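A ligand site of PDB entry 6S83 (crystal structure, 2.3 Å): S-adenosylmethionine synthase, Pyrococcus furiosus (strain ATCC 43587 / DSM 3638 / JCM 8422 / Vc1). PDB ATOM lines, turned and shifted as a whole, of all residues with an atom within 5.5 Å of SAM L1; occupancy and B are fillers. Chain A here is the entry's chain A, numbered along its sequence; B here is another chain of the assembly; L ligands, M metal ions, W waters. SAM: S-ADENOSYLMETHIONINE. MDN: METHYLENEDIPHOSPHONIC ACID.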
ATOM      1  N   HIS A  30     -18.276   6.315 -15.330  1.00  0.00           N
ATOM      2  CA  HIS A  30     -19.581   5.904 -15.825  1.00  0.00           C
ATOM      3  C   HIS A  30     -19.436   5.277 -17.211  1.00  0.00           C
ATOM      4  O   HIS A  30     -18.662   5.775 -18.041  1.00  0.00           O
ATOM      5  CB  HIS A  30     -20.514   7.110 -15.899  1.00  0.00           C
ATOM      6  CG  HIS A  30     -21.904   6.780 -16.331  1.00  0.00           C
ATOM      7  ND1 HIS A  30     -22.241   6.558 -17.646  1.00  0.00           N
ATOM      8  CD2 HIS A  30     -23.051   6.627 -15.621  1.00  0.00           C
ATOM      9  CE1 HIS A  30     -23.525   6.275 -17.733  1.00  0.00           C
ATOM     10  NE2 HIS A  30     -24.045   6.311 -16.509  1.00  0.00           N
ATOM     11  N   PRO A  31     -20.152   4.174 -17.499  1.00  0.00           N
ATOM     12  CA  PRO A  31     -19.945   3.497 -18.791  1.00  0.00           C
ATOM     13  C   PRO A  31     -20.040   4.413 -20.004  1.00  0.00           C
ATOM     14  O   PRO A  31     -19.192   4.351 -20.890  1.00  0.00           O
ATOM     15  CB  PRO A  31     -21.054   2.434 -18.796  1.00  0.00           C
ATOM     16  CG  PRO A  31     -21.326   2.168 -17.366  1.00  0.00           C
ATOM     17  CD  PRO A  31     -21.145   3.487 -16.665  1.00  0.00           C
ATOM     18  N   ASP A 198     -17.217   5.471 -11.119  1.00  0.00           N
ATOM     19  CA  ASP A 198     -18.559   5.513 -11.699  1.00  0.00           C
ATOM     20  C   ASP A 198     -19.445   6.328 -10.763  1.00  0.00           C
ATOM     21  O   ASP A 198     -20.183   5.802  -9.927  1.00  0.00           O
ATOM     22  CB  ASP A 198     -19.099   4.109 -11.945  1.00  0.00           C
ATOM     23  CG  ASP A 198     -20.441   4.111 -12.633  1.00  0.00           C
ATOM     24  OD1 ASP A 198     -21.009   5.195 -12.852  1.00  0.00           O
ATOM     25  OD2 ASP A 198     -20.923   3.008 -12.977  1.00  0.00           O
ATOM     26  N   ILE A 199     -19.358   7.642 -10.918  1.00  0.00           N
ATOM     27  CA  ILE A 199     -20.058   8.597 -10.077  1.00  0.00           C
ATOM     28  C   ILE A 199     -21.004   9.375 -10.956  1.00  0.00           C
ATOM     29  O   ILE A 199     -20.576  10.039 -11.908  1.00  0.00           O
ATOM     30  CB  ILE A 199     -19.076   9.530  -9.345  1.00  0.00           C
ATOM     31  CG1 ILE A 199     -18.179   8.705  -8.414  1.00  0.00           C
ATOM     32  CG2 ILE A 199     -19.835  10.615  -8.583  1.00  0.00           C
ATOM     33  CD1 ILE A 199     -17.102   9.492  -7.736  1.00  0.00           C
ATOM     34  N   LYS A 200     -22.298   9.288 -10.654  1.00  0.00           N
ATOM     35  CA  LYS A 200     -23.315  10.036 -11.367  1.00  0.00           C
ATOM     36  C   LYS A 200     -24.030  10.945 -10.371  1.00  0.00           C
ATOM     37  O   LYS A 200     -24.493  10.477  -9.326  1.00  0.00           O
ATOM     38  CB  LYS A 200     -24.307   9.089 -12.051  1.00  0.00           C
ATOM     39  CG  LYS A 200     -25.310   9.823 -12.919  1.00  0.00           C
ATOM     40  CD  LYS A 200     -26.059   8.873 -13.832  1.00  0.00           C
ATOM     41  CE  LYS A 200     -26.612   7.692 -13.085  1.00  0.00           C
ATOM     42  NZ  LYS A 200     -27.901   7.247 -13.677  1.00  0.00           N
ATOM     43  N   ALA A 215     -24.888   8.719  -7.194  1.00  0.00           N
ATOM     44  CA  ALA A 215     -24.716   7.291  -7.388  1.00  0.00           C
ATOM     45  C   ALA A 215     -23.233   7.033  -7.554  1.00  0.00           C
ATOM     46  O   ALA A 215     -22.640   7.418  -8.570  1.00  0.00           O
ATOM     47  CB  ALA A 215     -25.514   6.800  -8.597  1.00  0.00           C
ATOM     48  N   ASN A 257     -26.550   6.759  -3.255  1.00  0.00           N
ATOM     49  CA  ASN A 257     -26.941   5.389  -3.563  1.00  0.00           C
ATOM     50  C   ASN A 257     -28.309   5.052  -2.961  1.00  0.00           C
ATOM     51  O   ASN A 257     -28.456   4.268  -2.024  1.00  0.00           O
ATOM     52  CB  ASN A 257     -25.868   4.408  -3.062  1.00  0.00           C
ATOM     53  CG  ASN A 257     -24.509   4.694  -3.663  1.00  0.00           C
ATOM     54  OD1 ASN A 257     -24.389   5.393  -4.666  1.00  0.00           O
ATOM     55  ND2 ASN A 257     -23.464   4.150  -3.045  1.00  0.00           N
ATOM     56  N   THR A 258     -29.330   5.674  -3.554  1.00  0.00           N
ATOM     57  CA  THR A 258     -30.694   5.533  -3.080  1.00  0.00           C
ATOM     58  C   THR A 258     -31.253   4.137  -3.295  1.00  0.00           C
ATOM     59  O   THR A 258     -32.231   3.762  -2.640  1.00  0.00           O
ATOM     60  CB  THR A 258     -31.594   6.569  -3.761  1.00  0.00           C
ATOM     61  OG1 THR A 258     -31.060   7.882  -3.542  1.00  0.00           O
ATOM     62  CG2 THR A 258     -33.033   6.493  -3.237  1.00  0.00           C
ATOM     63  N   ALA A 259     -30.668   3.349  -4.201  1.00  0.00           N
ATOM     64  CA  ALA A 259     -31.168   2.004  -4.466  1.00  0.00           C
ATOM     65  C   ALA A 259     -30.813   1.007  -3.374  1.00  0.00           C
ATOM     66  O   ALA A 259     -31.334  -0.112  -3.397  1.00  0.00           O
ATOM     67  CB  ALA A 259     -30.628   1.502  -5.801  1.00  0.00           C
ATOM     68  N   ASP A 260     -29.961   1.385  -2.417  1.00  0.00           N
ATOM     69  CA  ASP A 260     -29.524   0.444  -1.393  1.00  0.00           C
ATOM     70  C   ASP A 260     -30.714  -0.062  -0.573  1.00  0.00           C
ATOM     71  O   ASP A 260     -31.649   0.682  -0.280  1.00  0.00           O
ATOM     72  CB  ASP A 260     -28.495   1.096  -0.476  1.00  0.00           C
ATOM     73  CG  ASP A 260     -27.167   1.310  -1.162  1.00  0.00           C
ATOM     74  OD1 ASP A 260     -26.991   0.833  -2.307  1.00  0.00           O
ATOM     75  OD2 ASP A 260     -26.282   1.957  -0.553  1.00  0.00           O
ATOM     76  N   TYR A 267     -26.603  -3.593  -2.227  1.00  0.00           N
ATOM     77  CA  TYR A 267     -25.587  -2.568  -2.017  1.00  0.00           C
ATOM     78  C   TYR A 267     -24.944  -2.232  -3.346  1.00  0.00           C
ATOM     79  O   TYR A 267     -24.775  -3.104  -4.205  1.00  0.00           O
ATOM     80  CB  TYR A 267     -24.518  -3.045  -1.021  1.00  0.00           C
ATOM     81  CG  TYR A 267     -25.055  -3.376   0.351  1.00  0.00           C
ATOM     82  CD1 TYR A 267     -25.948  -2.528   0.987  1.00  0.00           C
ATOM     83  CD2 TYR A 267     -24.692  -4.547   0.987  1.00  0.00           C
ATOM     84  CE1 TYR A 267     -26.438  -2.838   2.243  1.00  0.00           C
ATOM     85  CE2 TYR A 267     -25.177  -4.866   2.241  1.00  0.00           C
ATOM     86  CZ  TYR A 267     -26.052  -4.005   2.860  1.00  0.00           C
ATOM     87  OH  TYR A 267     -26.551  -4.318   4.105  1.00  0.00           O
ATOM     88  N   TYR A 268     -24.570  -0.965  -3.513  1.00  0.00           N
ATOM     89  CA  TYR A 268     -23.873  -0.539  -4.724  1.00  0.00           C
ATOM     90  C   TYR A 268     -22.365  -0.725  -4.541  1.00  0.00           C
ATOM     91  O   TYR A 268     -21.582   0.231  -4.470  1.00  0.00           O
ATOM     92  CB  TYR A 268     -24.228   0.900  -5.069  1.00  0.00           C
ATOM     93  CG  TYR A 268     -23.748   1.360  -6.431  1.00  0.00           C
ATOM     94  CD1 TYR A 268     -23.258   0.457  -7.370  1.00  0.00           C
ATOM     95  CD2 TYR A 268     -23.783   2.710  -6.785  1.00  0.00           C
ATOM     96  CE1 TYR A 268     -22.816   0.875  -8.607  1.00  0.00           C
ATOM     97  CE2 TYR A 268     -23.346   3.137  -8.021  1.00  0.00           C
ATOM     98  CZ  TYR A 268     -22.860   2.216  -8.933  1.00  0.00           C
ATOM     99  OH  TYR A 268     -22.427   2.630 -10.172  1.00  0.00           O
ATOM    100  N   SER A 275     -19.684   0.400 -12.806  1.00  0.00           N
ATOM    101  CA  SER A 275     -20.808  -0.486 -13.106  1.00  0.00           C
ATOM    102  C   SER A 275     -20.694  -1.120 -14.484  1.00  0.00           C
ATOM    103  O   SER A 275     -21.527  -1.967 -14.822  1.00  0.00           O
ATOM    104  CB  SER A 275     -22.129   0.270 -12.983  1.00  0.00           C
ATOM    105  OG  SER A 275     -22.248   1.236 -14.015  1.00  0.00           O
ATOM    106  N   GLY A 279     -23.915  -4.438 -14.552  1.00  0.00           N
ATOM    107  CA  GLY A 279     -25.241  -4.178 -15.073  1.00  0.00           C
ATOM    108  C   GLY A 279     -25.474  -2.903 -15.840  1.00  0.00           C
ATOM    109  O   GLY A 279     -26.641  -2.539 -16.045  1.00  0.00           O
ATOM    110  N   ASP A 280     -24.438  -2.190 -16.263  1.00  0.00           N
ATOM    111  CA  ASP A 280     -24.620  -1.032 -17.131  1.00  0.00           C
ATOM    112  C   ASP A 280     -23.693  -1.092 -18.330  1.00  0.00           C
ATOM    113  O   ASP A 280     -22.526  -1.499 -18.213  1.00  0.00           O
ATOM    114  CB  ASP A 280     -24.400   0.288 -16.378  1.00  0.00           C
ATOM    115  CG  ASP A 280     -24.952   1.481 -17.147  1.00  0.00           C
ATOM    116  OD1 ASP A 280     -25.810   1.273 -18.034  1.00  0.00           O
ATOM    117  OD2 ASP A 280     -24.527   2.623 -16.878  1.00  0.00           O
ATOM    118  N   ASP A 281     -24.227  -0.712 -19.483  1.00  0.00           N
ATOM    119  CA  ASP A 281     -23.486  -0.621 -20.741  1.00  0.00           C
ATOM    120  C   ASP A 281     -23.299   0.850 -21.100  1.00  0.00           C
ATOM    121  O   ASP A 281     -23.949   1.728 -20.544  1.00  0.00           O
ATOM    122  CB  ASP A 281     -24.235  -1.355 -21.849  1.00  0.00           C
ATOM    123  CG  ASP A 281     -24.525  -2.799 -21.508  1.00  0.00           C
ATOM    124  OD1 ASP A 281     -23.556  -3.576 -21.338  1.00  0.00           O
ATOM    125  OD2 ASP A 281     -25.714  -3.155 -21.392  1.00  0.00           O
ATOM    126  N   HIS B  59     -36.230  -8.520 -16.601  1.00  0.00           N
ATOM    127  CA  HIS B  59     -35.369  -7.356 -16.776  1.00  0.00           C
ATOM    128  C   HIS B  59     -34.576  -7.461 -18.077  1.00  0.00           C
ATOM    129  O   HIS B  59     -34.031  -8.513 -18.411  1.00  0.00           O
ATOM    130  CB  HIS B  59     -34.405  -7.217 -15.604  1.00  0.00           C
ATOM    131  CG  HIS B  59     -33.421  -6.113 -15.777  1.00  0.00           C
ATOM    132  ND1 HIS B  59     -32.155  -6.319 -16.283  1.00  0.00           N
ATOM    133  CD2 HIS B  59     -33.511  -4.785 -15.547  1.00  0.00           C
ATOM    134  CE1 HIS B  59     -31.507  -5.163 -16.342  1.00  0.00           C
ATOM    135  NE2 HIS B  59     -32.317  -4.217 -15.890  1.00  0.00           N
ATOM    136  N   HIS B  60     -34.523  -6.347 -18.806  1.00  0.00           N
ATOM    137  CA  HIS B  60     -33.720  -6.277 -20.015  1.00  0.00           C
ATOM    138  C   HIS B  60     -33.746  -4.855 -20.570  1.00  0.00           C
ATOM    139  O   HIS B  60     -34.810  -4.251 -20.701  1.00  0.00           O
ATOM    140  CB  HIS B  60     -34.245  -7.252 -21.079  1.00  0.00           C
ATOM    141  CG  HIS B  60     -35.583  -6.880 -21.622  1.00  0.00           C
ATOM    142  ND1 HIS B  60     -35.757  -5.910 -22.584  1.00  0.00           N
ATOM    143  CD2 HIS B  60     -36.832  -7.333 -21.321  1.00  0.00           C
ATOM    144  CE1 HIS B  60     -37.038  -5.791 -22.864  1.00  0.00           C
ATOM    145  NE2 HIS B  60     -37.720  -6.641 -22.113  1.00  0.00           N
ATOM    146  N   ASN B  61     -32.570  -4.326 -20.879  1.00  0.00           N
ATOM    147  CA  ASN B  61     -32.442  -3.040 -21.566  1.00  0.00           C
ATOM    148  C   ASN B  61     -31.463  -3.251 -22.719  1.00  0.00           C
ATOM    149  O   ASN B  61     -30.249  -3.340 -22.496  1.00  0.00           O
ATOM    150  CB  ASN B  61     -31.980  -1.941 -20.624  1.00  0.00           C
ATOM    151  CG  ASN B  61     -33.090  -1.452 -19.709  1.00  0.00           C
ATOM    152  OD1 ASN B  61     -33.971  -0.702 -20.125  1.00  0.00           O
ATOM    153  ND2 ASN B  61     -33.041  -1.862 -18.439  1.00  0.00           N
ATOM    154  N   ARG B  92     -28.649  -5.560 -21.803  1.00  0.00           N
ATOM    155  CA  ARG B  92     -28.867  -6.521 -20.726  1.00  0.00           C
ATOM    156  C   ARG B  92     -30.161  -7.264 -20.984  1.00  0.00           C
ATOM    157  O   ARG B  92     -31.124  -6.705 -21.496  1.00  0.00           O
ATOM    158  CB  ARG B  92     -28.956  -5.827 -19.348  1.00  0.00           C
ATOM    159  CG  ARG B  92     -27.839  -4.845 -19.031  1.00  0.00           C
ATOM    160  CD  ARG B  92     -26.538  -5.545 -18.648  1.00  0.00           C
ATOM    161  NE  ARG B  92     -25.682  -5.798 -19.811  1.00  0.00           N
ATOM    162  CZ  ARG B  92     -24.471  -6.321 -19.755  1.00  0.00           C
ATOM    163  NH1 ARG B  92     -23.925  -6.640 -18.580  1.00  0.00           N
ATOM    164  NH2 ARG B  92     -23.775  -6.498 -20.867  1.00  0.00           N
ATOM    165  N   SER B 139     -27.013  -6.650 -13.511  1.00  0.00           N
ATOM    166  CA  SER B 139     -26.371  -6.811 -12.215  1.00  0.00           C
ATOM    167  C   SER B 139     -27.370  -7.296 -11.163  1.00  0.00           C
ATOM    168  O   SER B 139     -28.551  -6.945 -11.188  1.00  0.00           O
ATOM    169  CB  SER B 139     -25.736  -5.504 -11.761  1.00  0.00           C
ATOM    170  OG  SER B 139     -26.719  -4.490 -11.595  1.00  0.00           O
ATOM    171  N   ASP B 141     -28.063  -6.421  -8.396  1.00  0.00           N
ATOM    172  CA  ASP B 141     -28.811  -5.394  -7.665  1.00  0.00           C
ATOM    173  C   ASP B 141     -29.827  -4.677  -8.546  1.00  0.00           C
ATOM    174  O   ASP B 141     -30.995  -4.549  -8.153  1.00  0.00           O
ATOM    175  CB  ASP B 141     -27.833  -4.388  -7.042  1.00  0.00           C
ATOM    176  CG  ASP B 141     -26.864  -3.812  -8.048  1.00  0.00           C
ATOM    177  OD1 ASP B 141     -26.507  -4.518  -9.016  1.00  0.00           O
ATOM    178  OD2 ASP B 141     -26.455  -2.639  -7.876  1.00  0.00           O
ATOM    179  N   LEU B 142     -29.416  -4.194  -9.712  1.00  0.00           N
ATOM    180  CA  LEU B 142     -30.358  -3.528 -10.601  1.00  0.00           C
ATOM    181  C   LEU B 142     -31.497  -4.449 -11.009  1.00  0.00           C
ATOM    182  O   LEU B 142     -32.631  -4.001 -11.199  1.00  0.00           O
ATOM    183  CB  LEU B 142     -29.629  -2.988 -11.832  1.00  0.00           C
ATOM    184  CG  LEU B 142     -28.649  -1.841 -11.570  1.00  0.00           C
ATOM    185  CD1 LEU B 142     -27.932  -1.460 -12.859  1.00  0.00           C
ATOM    186  CD2 LEU B 142     -29.353  -0.630 -10.978  1.00  0.00           C
ATOM    187  N   ASN B 158     -35.696   2.242 -12.035  1.00  0.00           N
ATOM    188  CA  ASN B 158     -34.402   1.561 -12.075  1.00  0.00           C
ATOM    189  C   ASN B 158     -33.226   2.533 -12.134  1.00  0.00           C
ATOM    190  O   ASN B 158     -32.085   2.088 -12.015  1.00  0.00           O
ATOM    191  CB  ASN B 158     -34.329   0.624 -13.282  1.00  0.00           C
ATOM    192  CG  ASN B 158     -34.493   1.347 -14.601  1.00  0.00           C
ATOM    193  OD1 ASN B 158     -34.599   2.575 -14.654  1.00  0.00           O
ATOM    194  ND2 ASN B 158     -34.499   0.578 -15.690  1.00  0.00           N
ATOM    195  N   ASP B 159     -33.473   3.822 -12.331  1.00  0.00           N
ATOM    196  CA  ASP B 159     -32.387   4.790 -12.383  1.00  0.00           C
ATOM    197  C   ASP B 159     -32.885   6.157 -11.922  1.00  0.00           C
ATOM    198  O   ASP B 159     -34.093   6.405 -11.833  1.00  0.00           O
ATOM    199  CB  ASP B 159     -31.816   4.895 -13.805  1.00  0.00           C
ATOM    200  CG  ASP B 159     -30.407   5.457 -13.819  1.00  0.00           C
ATOM    201  OD1 ASP B 159     -29.879   5.776 -12.737  1.00  0.00           O
ATOM    202  OD2 ASP B 159     -29.835   5.580 -14.922  1.00  0.00           O
ATOM    203  N   ASN B 309     -36.648  -1.183 -21.535  1.00  0.00           N
ATOM    204  CA  ASN B 309     -37.874  -1.879 -21.216  1.00  0.00           C
ATOM    205  C   ASN B 309     -38.961  -0.863 -20.849  1.00  0.00           C
ATOM    206  O   ASN B 309     -38.695   0.096 -20.128  1.00  0.00           O
ATOM    207  CB  ASN B 309     -37.672  -2.875 -20.075  1.00  0.00           C
ATOM    208  CG  ASN B 309     -37.464  -2.198 -18.734  1.00  0.00           C
ATOM    209  OD1 ASN B 309     -38.422  -1.817 -18.059  1.00  0.00           O
ATOM    210  ND2 ASN B 309     -36.216  -2.069 -18.320  1.00  0.00           N
ATOM    211  N   HIS B 313     -37.755   1.397 -16.916  1.00  0.00           N
ATOM    212  CA  HIS B 313     -36.759   2.389 -17.281  1.00  0.00           C
ATOM    213  C   HIS B 313     -37.436   3.729 -17.529  1.00  0.00           C
ATOM    214  O   HIS B 313     -38.307   3.845 -18.400  1.00  0.00           O
ATOM    215  CB  HIS B 313     -35.973   1.961 -18.526  1.00  0.00           C
ATOM    216  CG  HIS B 313     -34.623   2.581 -18.593  1.00  0.00           C
ATOM    217  ND1 HIS B 313     -34.433   3.955 -18.623  1.00  0.00           N
ATOM    218  CD2 HIS B 313     -33.386   2.032 -18.642  1.00  0.00           C
ATOM    219  CE1 HIS B 313     -33.145   4.215 -18.672  1.00  0.00           C
ATOM    220  NE2 HIS B 313     -32.485   3.072 -18.695  1.00  0.00           N
ATOM    221  N   ILE B 346     -34.039   6.672  -8.131  1.00  0.00           N
ATOM    222  CA  ILE B 346     -33.833   5.234  -8.286  1.00  0.00           C
ATOM    223  C   ILE B 346     -34.334   4.519  -7.050  1.00  0.00           C
ATOM    224  O   ILE B 346     -33.959   4.838  -5.921  1.00  0.00           O
ATOM    225  CB  ILE B 346     -32.358   4.913  -8.584  1.00  0.00           C
ATOM    226  CG1 ILE B 346     -32.210   3.417  -8.862  1.00  0.00           C
ATOM    227  CG2 ILE B 346     -31.459   5.353  -7.433  1.00  0.00           C
ATOM    228  CD1 ILE B 346     -30.839   2.991  -9.364  1.00  0.00           C
HETATM  229  N   SAM L   1     -28.489  -0.490 -17.576  1.00  0.00           N
HETATM  230  CA  SAM L   1     -29.251  -0.791 -16.365  1.00  0.00           C
HETATM  231  C   SAM L   1     -30.413  -1.729 -16.685  1.00  0.00           C
HETATM  232  O   SAM L   1     -30.351  -2.534 -17.606  1.00  0.00           O
HETATM  233  OXT SAM L   1     -31.439  -1.697 -16.001  1.00  0.00           O
HETATM  234  CB  SAM L   1     -29.765   0.478 -15.708  1.00  0.00           C
HETATM  235  CG  SAM L   1     -28.905   1.732 -15.796  1.00  0.00           C
HETATM  236  SD  SAM L   1     -27.792   1.947 -14.385  1.00  0.00           S
HETATM  237  CE  SAM L   1     -28.992   2.446 -13.125  1.00  0.00           C
HETATM  238  C5' SAM L   1     -27.068   3.525 -14.876  1.00  0.00           C
HETATM  239  C4' SAM L   1     -26.052   4.129 -13.917  1.00  0.00           C
HETATM  240  O4' SAM L   1     -26.538   4.120 -12.588  1.00  0.00           O
HETATM  241  C3' SAM L   1     -24.736   3.395 -13.905  1.00  0.00           C
HETATM  242  O3' SAM L   1     -23.839   3.944 -14.846  1.00  0.00           O
HETATM  243  C2' SAM L   1     -24.235   3.588 -12.500  1.00  0.00           C
HETATM  244  O2' SAM L   1     -23.356   4.690 -12.442  1.00  0.00           O
HETATM  245  C1' SAM L   1     -25.497   3.826 -11.683  1.00  0.00           C
HETATM  246  N9  SAM L   1     -25.890   2.635 -10.904  1.00  0.00           N
HETATM  247  C8  SAM L   1     -25.717   1.328 -11.271  1.00  0.00           C
HETATM  248  N7  SAM L   1     -26.205   0.535 -10.292  1.00  0.00           N
HETATM  249  C5  SAM L   1     -26.699   1.324  -9.302  1.00  0.00           C
HETATM  250  C6  SAM L   1     -27.304   1.027  -8.088  1.00  0.00           C
HETATM  251  N6  SAM L   1     -27.491  -0.247  -7.735  1.00  0.00           N
HETATM  252  N1  SAM L   1     -27.718   2.049  -7.269  1.00  0.00           N
HETATM  253  C2  SAM L   1     -27.518   3.370  -7.653  1.00  0.00           C
HETATM  254  N3  SAM L   1     -26.917   3.653  -8.861  1.00  0.00           N
HETATM  255  C4  SAM L   1     -26.512   2.648  -9.677  1.00  0.00           C
HETATM  256  O3  MDN L   2     -30.401   4.997 -19.666  1.00  0.00           O
HETATM  257  P1  MDN L   2     -29.284   4.007 -19.317  1.00  0.00           P
HETATM  258  O1  MDN L   2     -29.924   2.654 -19.008  1.00  0.00           O
HETATM  259  O2  MDN L   2     -28.256   3.805 -20.437  1.00  0.00           O
HETATM  260  C4  MDN L   2     -28.416   4.549 -17.762  1.00  0.00           C
HETATM  261  P5  MDN L   2     -27.371   6.100 -17.652  1.00  0.00           P
HETATM  262  O6  MDN L   2     -26.269   6.068 -18.711  1.00  0.00           O
HETATM  263  O7  MDN L   2     -28.255   7.345 -17.729  1.00  0.00           O
HETATM  264  O8  MDN L   2     -26.699   6.081 -16.271  1.00  0.00           O
HETATM  265 MG    MG M   1     -28.409   1.514 -21.783  1.00  0.00          MG
HETATM  266  O   HOH W   1     -22.702   5.130 -10.128  1.00  0.00           O
HETATM  267  O   HOH W   2     -25.273  -2.591 -10.725  1.00  0.00           O
HETATM  268  O   HOH W   3     -28.280   5.719 -10.641  1.00  0.00           O
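ND2 of Asn 61 of chain B lies within hydrogen-bond range of O of SAM L1 (2.9 Å). The backbone carbonyl oxygen (O) of Gly 279 is in hydrogen-bond range of a nitrogen (N) of SAM L1, at 3.2 Å. NE2 of His 313 of chain B is in hydrogen-bond range of O1 of MDN L2, 2.6 Å away. An oxygen (O2') of SAM L1 is in hydrogen-bond range of the side-chain carboxylate of Asp 198 (2.4 Å). A ring nitrogen (NE2) of His 30 sits at hydrogen-bond distance from an oxygen (O8) of MDN L2 (2.7 Å). OH of Tyr 268 lies close to O2' of SAM L1 (3.2 Å). The side-chain carboxylate (OD2) of Asp 141 of chain B is in hydrogen-bond range of a nitrogen (N6) of SAM L1, at 2.6 Å. O3' of SAM L1 lies within hydrogen-bond range of NE2 of His 30. An oxygen (O3') of SAM L1 sits at hydrogen-bond distance from the side-chain hydroxyl (OG) of Ser 275 (3.2 Å). An oxygen (O8) of MDN L2 is in salt-bridge range of the side-chain amino group of Lys 200, 3.1 Å away. A ring nitrogen (NE2) of His 59 of chain B is in hydrogen-bond range of an oxygen (OXT) of SAM L1 (2.7 Å). A nitrogen (N) of SAM L1 lies within salt-bridge range of the side-chain carboxylate (OD1) of Asp 280 (3.2 Å).
The side-chain hydroxyl of Ser 139 of chain B sits close to the backbone NH of Leu 142 of chain B, 3.3 Å away. N of Tyr 268 lies within hydrogen-bond range of OD1 of Asp 260, at 3.2 Å. OD1 of Asp 141 of chain B is in hydrogen-bond range of OG of Ser 139 of chain B, at 2.6 Å. The backbone carbonyl oxygen of Asn 61 of chain B is in hydrogen-bond range of the backbone NH of Arg 92 of chain B (2.8 Å). The backbone NH (N) of Ala 215 is in hydrogen-bond range of the backbone carbonyl oxygen (O) of Lys 200 (2.8 Å). The backbone NH of Asp 280 sits at hydrogen-bond distance from the backbone carbonyl oxygen of Ser 275 (3.3 Å). OD1 of Asp 159 of chain B is in salt-bridge range of NZ of Lys 200 (2.6 Å). The side-chain carboxylate (OD2) of Asp 198 sits at hydrogen-bond distance from the side-chain hydroxyl (OH) of Tyr 268 (3.2 Å).
Residues that only touch SAM L1: Pro 31 (3.3 Å), Lys 200 (3.6 Å), Ala 215 (3.5 Å), Ala 259 (3.3 Å), Arg 92 of chain B (3.7 Å), Leu 142 of chain B (3.4 Å), Asn 158 of chain B (3.3 Å), Asp 159 of chain B (3.4 Å) and Ile 346 of chain B (3.8 Å). Hydrophobic or aromatic side chains within 4 Å of SAM L1: His 30, Pro 31, Ala 215, Ala 259, Tyr 268, His 59 of chain B, Leu 142 of chain B and Ile 346 of chain B. Of the 28 residues printed, 18 come within 4 Å of SAM L1. The nearest printed residue that does not touch SAM L1 is Asn 257 (4.6 Å).
Water W1 lies within hydrogen-bond range of O2' of SAM L1 (2.4 Å), OH of Tyr 268 (2.5 Å), O of Asp 198 (2.6 Å) and O of Ala 215 (2.8 Å). Water W3 lies within hydrogen-bond range of the side-chain carboxylate of Asp 159 of chain B (2.6 Å), a nitrogen (N3) of SAM L1 (3.0 Å) and the side-chain amino group of Lys 200 (3.4 Å). Water W2 lies within hydrogen-bond range of the side-chain hydroxyl (OG) of Ser 139 of chain B (2.5 Å), the side-chain carboxylate (OD1) of Asp 141 of chain B (2.9 Å) and a nitrogen (N7) of SAM L1 (3.3 Å).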
